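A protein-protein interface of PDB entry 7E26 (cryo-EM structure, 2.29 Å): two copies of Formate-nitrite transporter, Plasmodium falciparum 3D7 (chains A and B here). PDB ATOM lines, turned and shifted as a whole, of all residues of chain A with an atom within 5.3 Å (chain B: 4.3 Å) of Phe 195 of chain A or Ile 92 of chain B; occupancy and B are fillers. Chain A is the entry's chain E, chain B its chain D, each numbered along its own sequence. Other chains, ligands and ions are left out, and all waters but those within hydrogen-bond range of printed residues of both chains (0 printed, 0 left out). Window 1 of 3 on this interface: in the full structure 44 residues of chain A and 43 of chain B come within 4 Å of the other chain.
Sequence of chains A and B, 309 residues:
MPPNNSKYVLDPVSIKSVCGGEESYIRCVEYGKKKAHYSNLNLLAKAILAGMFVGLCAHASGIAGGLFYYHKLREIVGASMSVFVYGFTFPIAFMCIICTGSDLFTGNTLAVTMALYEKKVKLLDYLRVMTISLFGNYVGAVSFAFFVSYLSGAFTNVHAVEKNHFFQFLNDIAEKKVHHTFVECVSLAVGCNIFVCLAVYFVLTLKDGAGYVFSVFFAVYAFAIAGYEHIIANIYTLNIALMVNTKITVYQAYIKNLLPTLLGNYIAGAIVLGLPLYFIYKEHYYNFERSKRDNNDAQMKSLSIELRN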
ATOM      1  N   VAL A 190      -8.423  30.799  -1.834  1.00  0.00           N
ATOM      2  CA  VAL A 190      -8.074  29.976  -2.990  1.00  0.00           C
ATOM      3  C   VAL A 190      -9.006  28.773  -3.089  1.00  0.00           C
ATOM      4  O   VAL A 190      -9.568  28.485  -4.162  1.00  0.00           O
ATOM      5  CB  VAL A 190      -6.594  29.552  -2.914  1.00  0.00           C
ATOM      6  CG1 VAL A 190      -6.302  28.419  -3.871  1.00  0.00           C
ATOM      7  CG2 VAL A 190      -5.686  30.718  -3.226  1.00  0.00           C
ATOM      8  N   GLY A 191      -9.216  28.081  -1.965  1.00  0.00           N
ATOM      9  CA  GLY A 191     -10.163  26.981  -1.926  1.00  0.00           C
ATOM     10  C   GLY A 191     -11.591  27.369  -2.252  1.00  0.00           C
ATOM     11  O   GLY A 191     -12.324  26.554  -2.820  1.00  0.00           O
ATOM     12  N   CYS A 192     -11.996  28.598  -1.919  1.00  0.00           N
ATOM     13  CA  CYS A 192     -13.325  29.070  -2.302  1.00  0.00           C
ATOM     14  C   CYS A 192     -13.447  29.295  -3.800  1.00  0.00           C
ATOM     15  O   CYS A 192     -14.421  28.857  -4.435  1.00  0.00           O
ATOM     16  CB  CYS A 192     -13.650  30.368  -1.588  1.00  0.00           C
ATOM     17  SG  CYS A 192     -15.195  31.044  -2.138  1.00  0.00           S
ATOM     18  N   ASN A 193     -12.504  30.040  -4.372  1.00  0.00           N
ATOM     19  CA  ASN A 193     -12.691  30.430  -5.758  1.00  0.00           C
ATOM     20  C   ASN A 193     -12.455  29.292  -6.734  1.00  0.00           C
ATOM     21  O   ASN A 193     -12.938  29.383  -7.869  1.00  0.00           O
ATOM     22  CB  ASN A 193     -11.808  31.613  -6.128  1.00  0.00           C
ATOM     23  CG  ASN A 193     -12.421  32.447  -7.216  1.00  0.00           C
ATOM     24  OD1 ASN A 193     -13.632  32.449  -7.378  1.00  0.00           O
ATOM     25  ND2 ASN A 193     -11.597  33.138  -7.983  1.00  0.00           N
ATOM     26  N   ILE A 194     -11.776  28.216  -6.319  1.00  0.00           N
ATOM     27  CA  ILE A 194     -11.764  27.023  -7.164  1.00  0.00           C
ATOM     28  C   ILE A 194     -13.178  26.452  -7.317  1.00  0.00           C
ATOM     29  O   ILE A 194     -13.613  26.157  -8.438  1.00  0.00           O
ATOM     30  CB  ILE A 194     -10.765  25.981  -6.632  1.00  0.00           C
ATOM     31  CG1 ILE A 194      -9.341  26.512  -6.748  1.00  0.00           C
ATOM     32  CG2 ILE A 194     -10.820  24.734  -7.459  1.00  0.00           C
ATOM     33  CD1 ILE A 194      -8.342  25.734  -5.950  1.00  0.00           C
ATOM     34  N   PHE A 195     -13.938  26.350  -6.214  1.00  0.00           N
ATOM     35  CA  PHE A 195     -15.340  25.931  -6.296  1.00  0.00           C
ATOM     36  C   PHE A 195     -16.204  26.895  -7.100  1.00  0.00           C
ATOM     37  O   PHE A 195     -17.083  26.452  -7.846  1.00  0.00           O
ATOM     38  CB  PHE A 195     -15.974  25.777  -4.910  1.00  0.00           C
ATOM     39  CG  PHE A 195     -15.699  24.467  -4.240  1.00  0.00           C
ATOM     40  CD1 PHE A 195     -16.233  23.297  -4.751  1.00  0.00           C
ATOM     41  CD2 PHE A 195     -15.012  24.412  -3.043  1.00  0.00           C
ATOM     42  CE1 PHE A 195     -16.015  22.092  -4.126  1.00  0.00           C
ATOM     43  CE2 PHE A 195     -14.805  23.207  -2.408  1.00  0.00           C
ATOM     44  CZ  PHE A 195     -15.303  22.048  -2.953  1.00  0.00           C
ATOM     45  N   VAL A 196     -15.988  28.204  -6.955  1.00  0.00           N
ATOM     46  CA  VAL A 196     -16.843  29.166  -7.657  1.00  0.00           C
ATOM     47  C   VAL A 196     -16.591  29.134  -9.168  1.00  0.00           C
ATOM     48  O   VAL A 196     -17.540  29.114  -9.974  1.00  0.00           O
ATOM     49  CB  VAL A 196     -16.650  30.573  -7.062  1.00  0.00           C
ATOM     50  CG1 VAL A 196     -17.367  31.616  -7.887  1.00  0.00           C
ATOM     51  CG2 VAL A 196     -17.169  30.604  -5.641  1.00  0.00           C
ATOM     52  N   CYS A 197     -15.321  29.082  -9.577  1.00  0.00           N
ATOM     53  CA  CYS A 197     -14.997  28.963 -10.991  1.00  0.00           C
ATOM     54  C   CYS A 197     -15.427  27.621 -11.574  1.00  0.00           C
ATOM     55  O   CYS A 197     -15.857  27.570 -12.733  1.00  0.00           O
ATOM     56  CB  CYS A 197     -13.501  29.182 -11.189  1.00  0.00           C
ATOM     57  SG  CYS A 197     -12.951  30.847 -10.806  1.00  0.00           S
ATOM     58  N   LEU A 198     -15.368  26.542 -10.790  1.00  0.00           N
ATOM     59  CA  LEU A 198     -15.906  25.272 -11.258  1.00  0.00           C
ATOM     60  C   LEU A 198     -17.424  25.291 -11.379  1.00  0.00           C
ATOM     61  O   LEU A 198     -17.968  24.603 -12.241  1.00  0.00           O
ATOM     62  CB  LEU A 198     -15.461  24.143 -10.333  1.00  0.00           C
ATOM     63  CG  LEU A 198     -14.046  23.671 -10.635  1.00  0.00           C
ATOM     64  CD1 LEU A 198     -13.475  22.985  -9.433  1.00  0.00           C
ATOM     65  CD2 LEU A 198     -14.090  22.728 -11.805  1.00  0.00           C
ATOM     66  N   ALA A 199     -18.119  26.077 -10.556  1.00  0.00           N
ATOM     67  CA  ALA A 199     -19.562  26.236 -10.730  1.00  0.00           C
ATOM     68  C   ALA A 199     -19.900  26.993 -12.010  1.00  0.00           C
ATOM     69  O   ALA A 199     -20.887  26.664 -12.686  1.00  0.00           O
ATOM     70  CB  ALA A 199     -20.159  26.945  -9.518  1.00  0.00           C
ATOM     71  N   VAL A 200     -19.095  28.001 -12.355  1.00  0.00           N
ATOM     72  CA  VAL A 200     -19.246  28.682 -13.644  1.00  0.00           C
ATOM     73  C   VAL A 200     -19.006  27.711 -14.803  1.00  0.00           C
ATOM     74  O   VAL A 200     -19.747  27.702 -15.800  1.00  0.00           O
ATOM     75  CB  VAL A 200     -18.296  29.894 -13.698  1.00  0.00           C
ATOM     76  CG1 VAL A 200     -18.236  30.497 -15.090  1.00  0.00           C
ATOM     77  CG2 VAL A 200     -18.733  30.935 -12.688  1.00  0.00           C
ATOM     78  N   PHE A 202     -19.499  24.482 -14.662  1.00  0.00           N
ATOM     79  CA  PHE A 202     -20.669  23.605 -14.669  1.00  0.00           C
ATOM     80  C   PHE A 202     -21.840  24.229 -15.410  1.00  0.00           C
ATOM     81  O   PHE A 202     -22.575  23.521 -16.102  1.00  0.00           O
ATOM     82  CB  PHE A 202     -21.127  23.282 -13.243  1.00  0.00           C
ATOM     83  CG  PHE A 202     -20.165  22.447 -12.444  1.00  0.00           C
ATOM     84  CD1 PHE A 202     -19.195  21.676 -13.057  1.00  0.00           C
ATOM     85  CD2 PHE A 202     -20.241  22.438 -11.059  1.00  0.00           C
ATOM     86  CE1 PHE A 202     -18.318  20.920 -12.305  1.00  0.00           C
ATOM     87  CE2 PHE A 202     -19.369  21.680 -10.307  1.00  0.00           C
ATOM     88  CZ  PHE A 202     -18.407  20.924 -10.931  1.00  0.00           C
ATOM     89  N   SER A 215     -25.610  20.829  -9.723  1.00  0.00           N
ATOM     90  CA  SER A 215     -24.155  20.938  -9.735  1.00  0.00           C
ATOM     91  C   SER A 215     -23.691  22.206  -9.033  1.00  0.00           C
ATOM     92  O   SER A 215     -22.761  22.161  -8.215  1.00  0.00           O
ATOM     93  CB  SER A 215     -23.638  20.896 -11.171  1.00  0.00           C
ATOM     94  OG  SER A 215     -24.180  21.950 -11.942  1.00  0.00           O
ATOM     95  N   PHE A 218     -24.360  21.704  -5.141  1.00  0.00           N
ATOM     96  CA  PHE A 218     -23.331  20.949  -4.440  1.00  0.00           C
ATOM     97  C   PHE A 218     -22.003  21.691  -4.389  1.00  0.00           C
ATOM     98  O   PHE A 218     -21.358  21.693  -3.333  1.00  0.00           O
ATOM     99  CB  PHE A 218     -23.159  19.578  -5.092  1.00  0.00           C
ATOM    100  CG  PHE A 218     -24.207  18.581  -4.687  1.00  0.00           C
ATOM    101  CD1 PHE A 218     -24.355  18.212  -3.361  1.00  0.00           C
ATOM    102  CD2 PHE A 218     -25.040  18.009  -5.631  1.00  0.00           C
ATOM    103  CE1 PHE A 218     -25.316  17.298  -2.988  1.00  0.00           C
ATOM    104  CE2 PHE A 218     -26.005  17.096  -5.263  1.00  0.00           C
ATOM    105  CZ  PHE A 218     -26.140  16.739  -3.940  1.00  0.00           C
ATOM    106  N   ALA A 219     -21.618  22.383  -5.466  1.00  0.00           N
ATOM    107  CA  ALA A 219     -20.382  23.157  -5.478  1.00  0.00           C
ATOM    108  C   ALA A 219     -20.404  24.345  -4.522  1.00  0.00           C
ATOM    109  O   ALA A 219     -19.377  24.660  -3.915  1.00  0.00           O
ATOM    110  CB  ALA A 219     -20.088  23.651  -6.895  1.00  0.00           C
ATOM    111  N   ALA A 222     -20.553  23.099  -0.848  1.00  0.00           N
ATOM    112  CA  ALA A 222     -19.272  22.548  -0.438  1.00  0.00           C
ATOM    113  C   ALA A 222     -18.301  23.614   0.054  1.00  0.00           C
ATOM    114  O   ALA A 222     -17.510  23.331   0.956  1.00  0.00           O
ATOM    115  CB  ALA A 222     -18.656  21.756  -1.585  1.00  0.00           C
ATOM    116  N   PHE A 223     -18.328  24.835  -0.490  1.00  0.00           N
ATOM    117  CA  PHE A 223     -17.460  25.829   0.129  1.00  0.00           C
ATOM    118  C   PHE A 223     -18.166  26.595   1.235  1.00  0.00           C
ATOM    119  O   PHE A 223     -17.488  27.197   2.072  1.00  0.00           O
ATOM    120  CB  PHE A 223     -16.831  26.803  -0.895  1.00  0.00           C
ATOM    121  CG  PHE A 223     -17.734  27.907  -1.411  1.00  0.00           C
ATOM    122  CD1 PHE A 223     -17.809  29.142  -0.760  1.00  0.00           C
ATOM    123  CD2 PHE A 223     -18.422  27.754  -2.593  1.00  0.00           C
ATOM    124  CE1 PHE A 223     -18.607  30.151  -1.234  1.00  0.00           C
ATOM    125  CE2 PHE A 223     -19.209  28.780  -3.085  1.00  0.00           C
ATOM    126  CZ  PHE A 223     -19.306  29.971  -2.399  1.00  0.00           C
ATOM    127  N   TYR A 228     -14.577  28.232   3.587  1.00  0.00           N
ATOM    128  CA  TYR A 228     -13.838  28.929   2.550  1.00  0.00           C
ATOM    129  C   TYR A 228     -14.367  30.353   2.393  1.00  0.00           C
ATOM    130  O   TYR A 228     -15.523  30.642   2.705  1.00  0.00           O
ATOM    131  CB  TYR A 228     -13.963  28.170   1.234  1.00  0.00           C
ATOM    132  CG  TYR A 228     -13.170  26.888   1.126  1.00  0.00           C
ATOM    133  CD1 TYR A 228     -11.971  26.719   1.802  1.00  0.00           C
ATOM    134  CD2 TYR A 228     -13.614  25.854   0.318  1.00  0.00           C
ATOM    135  CE1 TYR A 228     -11.250  25.549   1.686  1.00  0.00           C
ATOM    136  CE2 TYR A 228     -12.907  24.686   0.200  1.00  0.00           C
ATOM    137  CZ  TYR A 228     -11.730  24.536   0.880  1.00  0.00           C
ATOM    138  OH  TYR A 228     -11.034  23.363   0.745  1.00  0.00           O
ATOM    139  N   LEU B  56      -9.413  19.196  -2.606  1.00  0.00           N
ATOM    140  CA  LEU B  56     -10.355  20.281  -2.332  1.00  0.00           C
ATOM    141  C   LEU B  56     -11.626  19.779  -1.667  1.00  0.00           C
ATOM    142  O   LEU B  56     -12.009  20.247  -0.579  1.00  0.00           O
ATOM    143  CB  LEU B  56     -10.701  20.980  -3.644  1.00  0.00           C
ATOM    144  CG  LEU B  56     -11.720  22.119  -3.668  1.00  0.00           C
ATOM    145  CD1 LEU B  56     -11.192  23.434  -3.121  1.00  0.00           C
ATOM    146  CD2 LEU B  56     -12.318  22.280  -5.050  1.00  0.00           C
ATOM    147  N   CYS B  57     -12.288  18.823  -2.296  1.00  0.00           N
ATOM    148  CA  CYS B  57     -13.544  18.364  -1.735  1.00  0.00           C
ATOM    149  C   CYS B  57     -13.361  17.457  -0.529  1.00  0.00           C
ATOM    150  O   CYS B  57     -14.271  17.372   0.298  1.00  0.00           O
ATOM    151  CB  CYS B  57     -14.368  17.700  -2.822  1.00  0.00           C
ATOM    152  SG  CYS B  57     -14.451  18.780  -4.257  1.00  0.00           S
ATOM    153  N   THR B  89     -20.961  15.567   1.462  1.00  0.00           N
ATOM    154  CA  THR B  89     -20.191  16.690   0.940  1.00  0.00           C
ATOM    155  C   THR B  89     -19.202  16.246  -0.135  1.00  0.00           C
ATOM    156  O   THR B  89     -18.900  17.012  -1.058  1.00  0.00           O
ATOM    157  CB  THR B  89     -19.473  17.386   2.101  1.00  0.00           C
ATOM    158  OG1 THR B  89     -20.416  17.642   3.144  1.00  0.00           O
ATOM    159  CG2 THR B  89     -18.896  18.720   1.677  1.00  0.00           C
ATOM    160  N   PHE B  90     -18.717  15.005  -0.061  1.00  0.00           N
ATOM    161  CA  PHE B  90     -17.646  14.570  -0.960  1.00  0.00           C
ATOM    162  C   PHE B  90     -17.939  14.466  -2.467  1.00  0.00           C
ATOM    163  O   PHE B  90     -17.051  14.870  -3.236  1.00  0.00           O
ATOM    164  CB  PHE B  90     -17.076  13.237  -0.468  1.00  0.00           C
ATOM    165  CG  PHE B  90     -15.739  12.913  -1.062  1.00  0.00           C
ATOM    166  CD1 PHE B  90     -14.690  13.806  -0.945  1.00  0.00           C
ATOM    167  CD2 PHE B  90     -15.536  11.737  -1.759  1.00  0.00           C
ATOM    168  CE1 PHE B  90     -13.460  13.528  -1.500  1.00  0.00           C
ATOM    169  CE2 PHE B  90     -14.305  11.452  -2.316  1.00  0.00           C
ATOM    170  CZ  PHE B  90     -13.266  12.353  -2.186  1.00  0.00           C
ATOM    171  N   PRO B  91     -19.073  13.934  -2.967  1.00  0.00           N
ATOM    172  CA  PRO B  91     -19.123  13.524  -4.386  1.00  0.00           C
ATOM    173  C   PRO B  91     -19.054  14.625  -5.441  1.00  0.00           C
ATOM    174  O   PRO B  91     -19.136  14.301  -6.629  1.00  0.00           O
ATOM    175  CB  PRO B  91     -20.477  12.812  -4.485  1.00  0.00           C
ATOM    176  CG  PRO B  91     -20.763  12.376  -3.149  1.00  0.00           C
ATOM    177  CD  PRO B  91     -20.321  13.497  -2.313  1.00  0.00           C
ATOM    178  N   ILE B  92     -18.898  15.901  -5.086  1.00  0.00           N
ATOM    179  CA  ILE B  92     -18.763  16.938  -6.103  1.00  0.00           C
ATOM    180  C   ILE B  92     -17.373  16.953  -6.731  1.00  0.00           C
ATOM    181  O   ILE B  92     -17.190  17.555  -7.797  1.00  0.00           O
ATOM    182  CB  ILE B  92     -19.168  18.291  -5.474  1.00  0.00           C
ATOM    183  CG1 ILE B  92     -19.558  19.329  -6.535  1.00  0.00           C
ATOM    184  CG2 ILE B  92     -18.089  18.819  -4.559  1.00  0.00           C
ATOM    185  CD1 ILE B  92     -20.590  18.850  -7.529  1.00  0.00           C
ATOM    186  N   ALA B  93     -16.403  16.256  -6.120  1.00  0.00           N
ATOM    187  CA  ALA B  93     -15.046  16.174  -6.656  1.00  0.00           C
ATOM    188  C   ALA B  93     -15.006  15.502  -8.011  1.00  0.00           C
ATOM    189  O   ALA B  93     -14.256  15.923  -8.896  1.00  0.00           O
ATOM    190  CB  ALA B  93     -14.144  15.406  -5.694  1.00  0.00           C
ATOM    191  N   PHE B  94     -15.858  14.526  -8.211  1.00  0.00           N
ATOM    192  CA  PHE B  94     -15.946  13.778  -9.423  1.00  0.00           C
ATOM    193  C   PHE B  94     -16.556  14.551 -10.506  1.00  0.00           C
ATOM    194  O   PHE B  94     -16.192  14.428 -11.599  1.00  0.00           O
ATOM    195  CB  PHE B  94     -16.558  12.450  -9.135  1.00  0.00           C
ATOM    196  CG  PHE B  94     -15.739  11.676  -8.181  1.00  0.00           C
ATOM    197  CD1 PHE B  94     -15.821  11.920  -6.847  1.00  0.00           C
ATOM    198  CD2 PHE B  94     -14.784  10.822  -8.618  1.00  0.00           C
ATOM    199  CE1 PHE B  94     -15.013  11.272  -5.969  1.00  0.00           C
ATOM    200  CE2 PHE B  94     -13.971  10.165  -7.737  1.00  0.00           C
ATOM    201  CZ  PHE B  94     -14.086  10.391  -6.414  1.00  0.00           C
ATOM    202  N   MET B  95     -17.489  15.389 -10.189  1.00  0.00           N
ATOM    203  CA  MET B  95     -18.033  16.348 -11.139  1.00  0.00           C
ATOM    204  C   MET B  95     -17.007  17.390 -11.552  1.00  0.00           C
ATOM    205  O   MET B  95     -16.938  17.747 -12.734  1.00  0.00           O
ATOM    206  CB  MET B  95     -19.258  17.032 -10.537  1.00  0.00           C
ATOM    207  CG  MET B  95     -20.069  17.856 -11.517  1.00  0.00           C
ATOM    208  SD  MET B  95     -20.689  16.890 -12.896  1.00  0.00           S
ATOM    209  CE  MET B  95     -21.506  15.586 -12.001  1.00  0.00           C
ATOM    210  N   CYS B  96     -16.211  17.879 -10.595  1.00  0.00           N
ATOM    211  CA  CYS B  96     -15.122  18.800 -10.915  1.00  0.00           C
ATOM    212  C   CYS B  96     -14.073  18.152 -11.813  1.00  0.00           C
ATOM    213  O   CYS B  96     -13.497  18.823 -12.673  1.00  0.00           O
ATOM    214  CB  CYS B  96     -14.462  19.307  -9.633  1.00  0.00           C
ATOM    215  SG  CYS B  96     -15.549  20.174  -8.492  1.00  0.00           S
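The side-chain sulfur (SG) of Cys 57 of chain B lies close to the backbone NH (N) of Ala 93 of chain B, 3.7 Å away. The backbone carbonyl oxygen (O) of Phe 223 of chain A is in hydrogen-bond range of the backbone NH (N) of Tyr 228 of chain A, at 3.4 Å. O of Ile 92 of chain B is in hydrogen-bond range of SG of Cys 96 of chain B.
Among the printed residues, merely in contact across the chains: Gly 191 of chain A with Leu 56 of chain B, Ile 194 of chain A with Leu 56 of chain B, Phe 195 of chain A with Leu 56 of chain B, Phe 195 of chain A with Cys 57 of chain B, Phe 195 of chain A with Ile 92 of chain B, Leu 198 of chain A with Cys 96 of chain B, Phe 202 of chain A with Met 95 of chain B, Phe 202 of chain A with Cys 96 of chain B, Phe 218 of chain A with Ile 92 of chain B, Ala 219 of chain A with Ile 92 of chain B and Tyr 228 of chain A with Leu 56 of chain B.
Phe 195 of chain A touches just these residues of chain B: Leu 56, Cys 57 and Ile 92. Of the printed residues of chain A, Ile 92 of chain B touches Phe 195, Phe 218 and Ala 219. Of the printed residues of chain B, Gly 191 of chain A touches Leu 56. Of the printed residues of chain A, Cys 96 of chain B touches Leu 198 and Phe 202. Val 190 of chain A touches none of the printed residues of chain B. Ser 215 of chain A touches none of the printed residues of chain B. The nearest printed residue of chain A that does not touch Ile 92 of chain B is Ser 215 of chain A (4.02 Å).
Hydrophobic or aromatic side chains of chain B within 4 Å of the printed part of chain A: Leu 56, Ile 92 and Met 95. Of the 18 printed residues of chain A, 8 touch a printed residue of chain B. Printed residues of chain A that touch a printed residue of chain B: Gly 191, Ile 194, Phe 195, Leu 198, Phe 202, Phe 218, Ala 219 and Tyr 228. Hydrophobic or aromatic side chains of chain A within 4 Å of the printed part of chain B: Ile 194, Phe 195, Leu 198, Phe 202, Phe 218 and Tyr 228. Among the printed residues, no Asp or Glu carboxylate lies within 4 Å of a Lys or Arg side-chain nitrogen of the other chain.
No position is printed for both chains. Of the 11 pairs that touch across the chains among the printed residues, none has its exchanged pair printed and touching as well.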
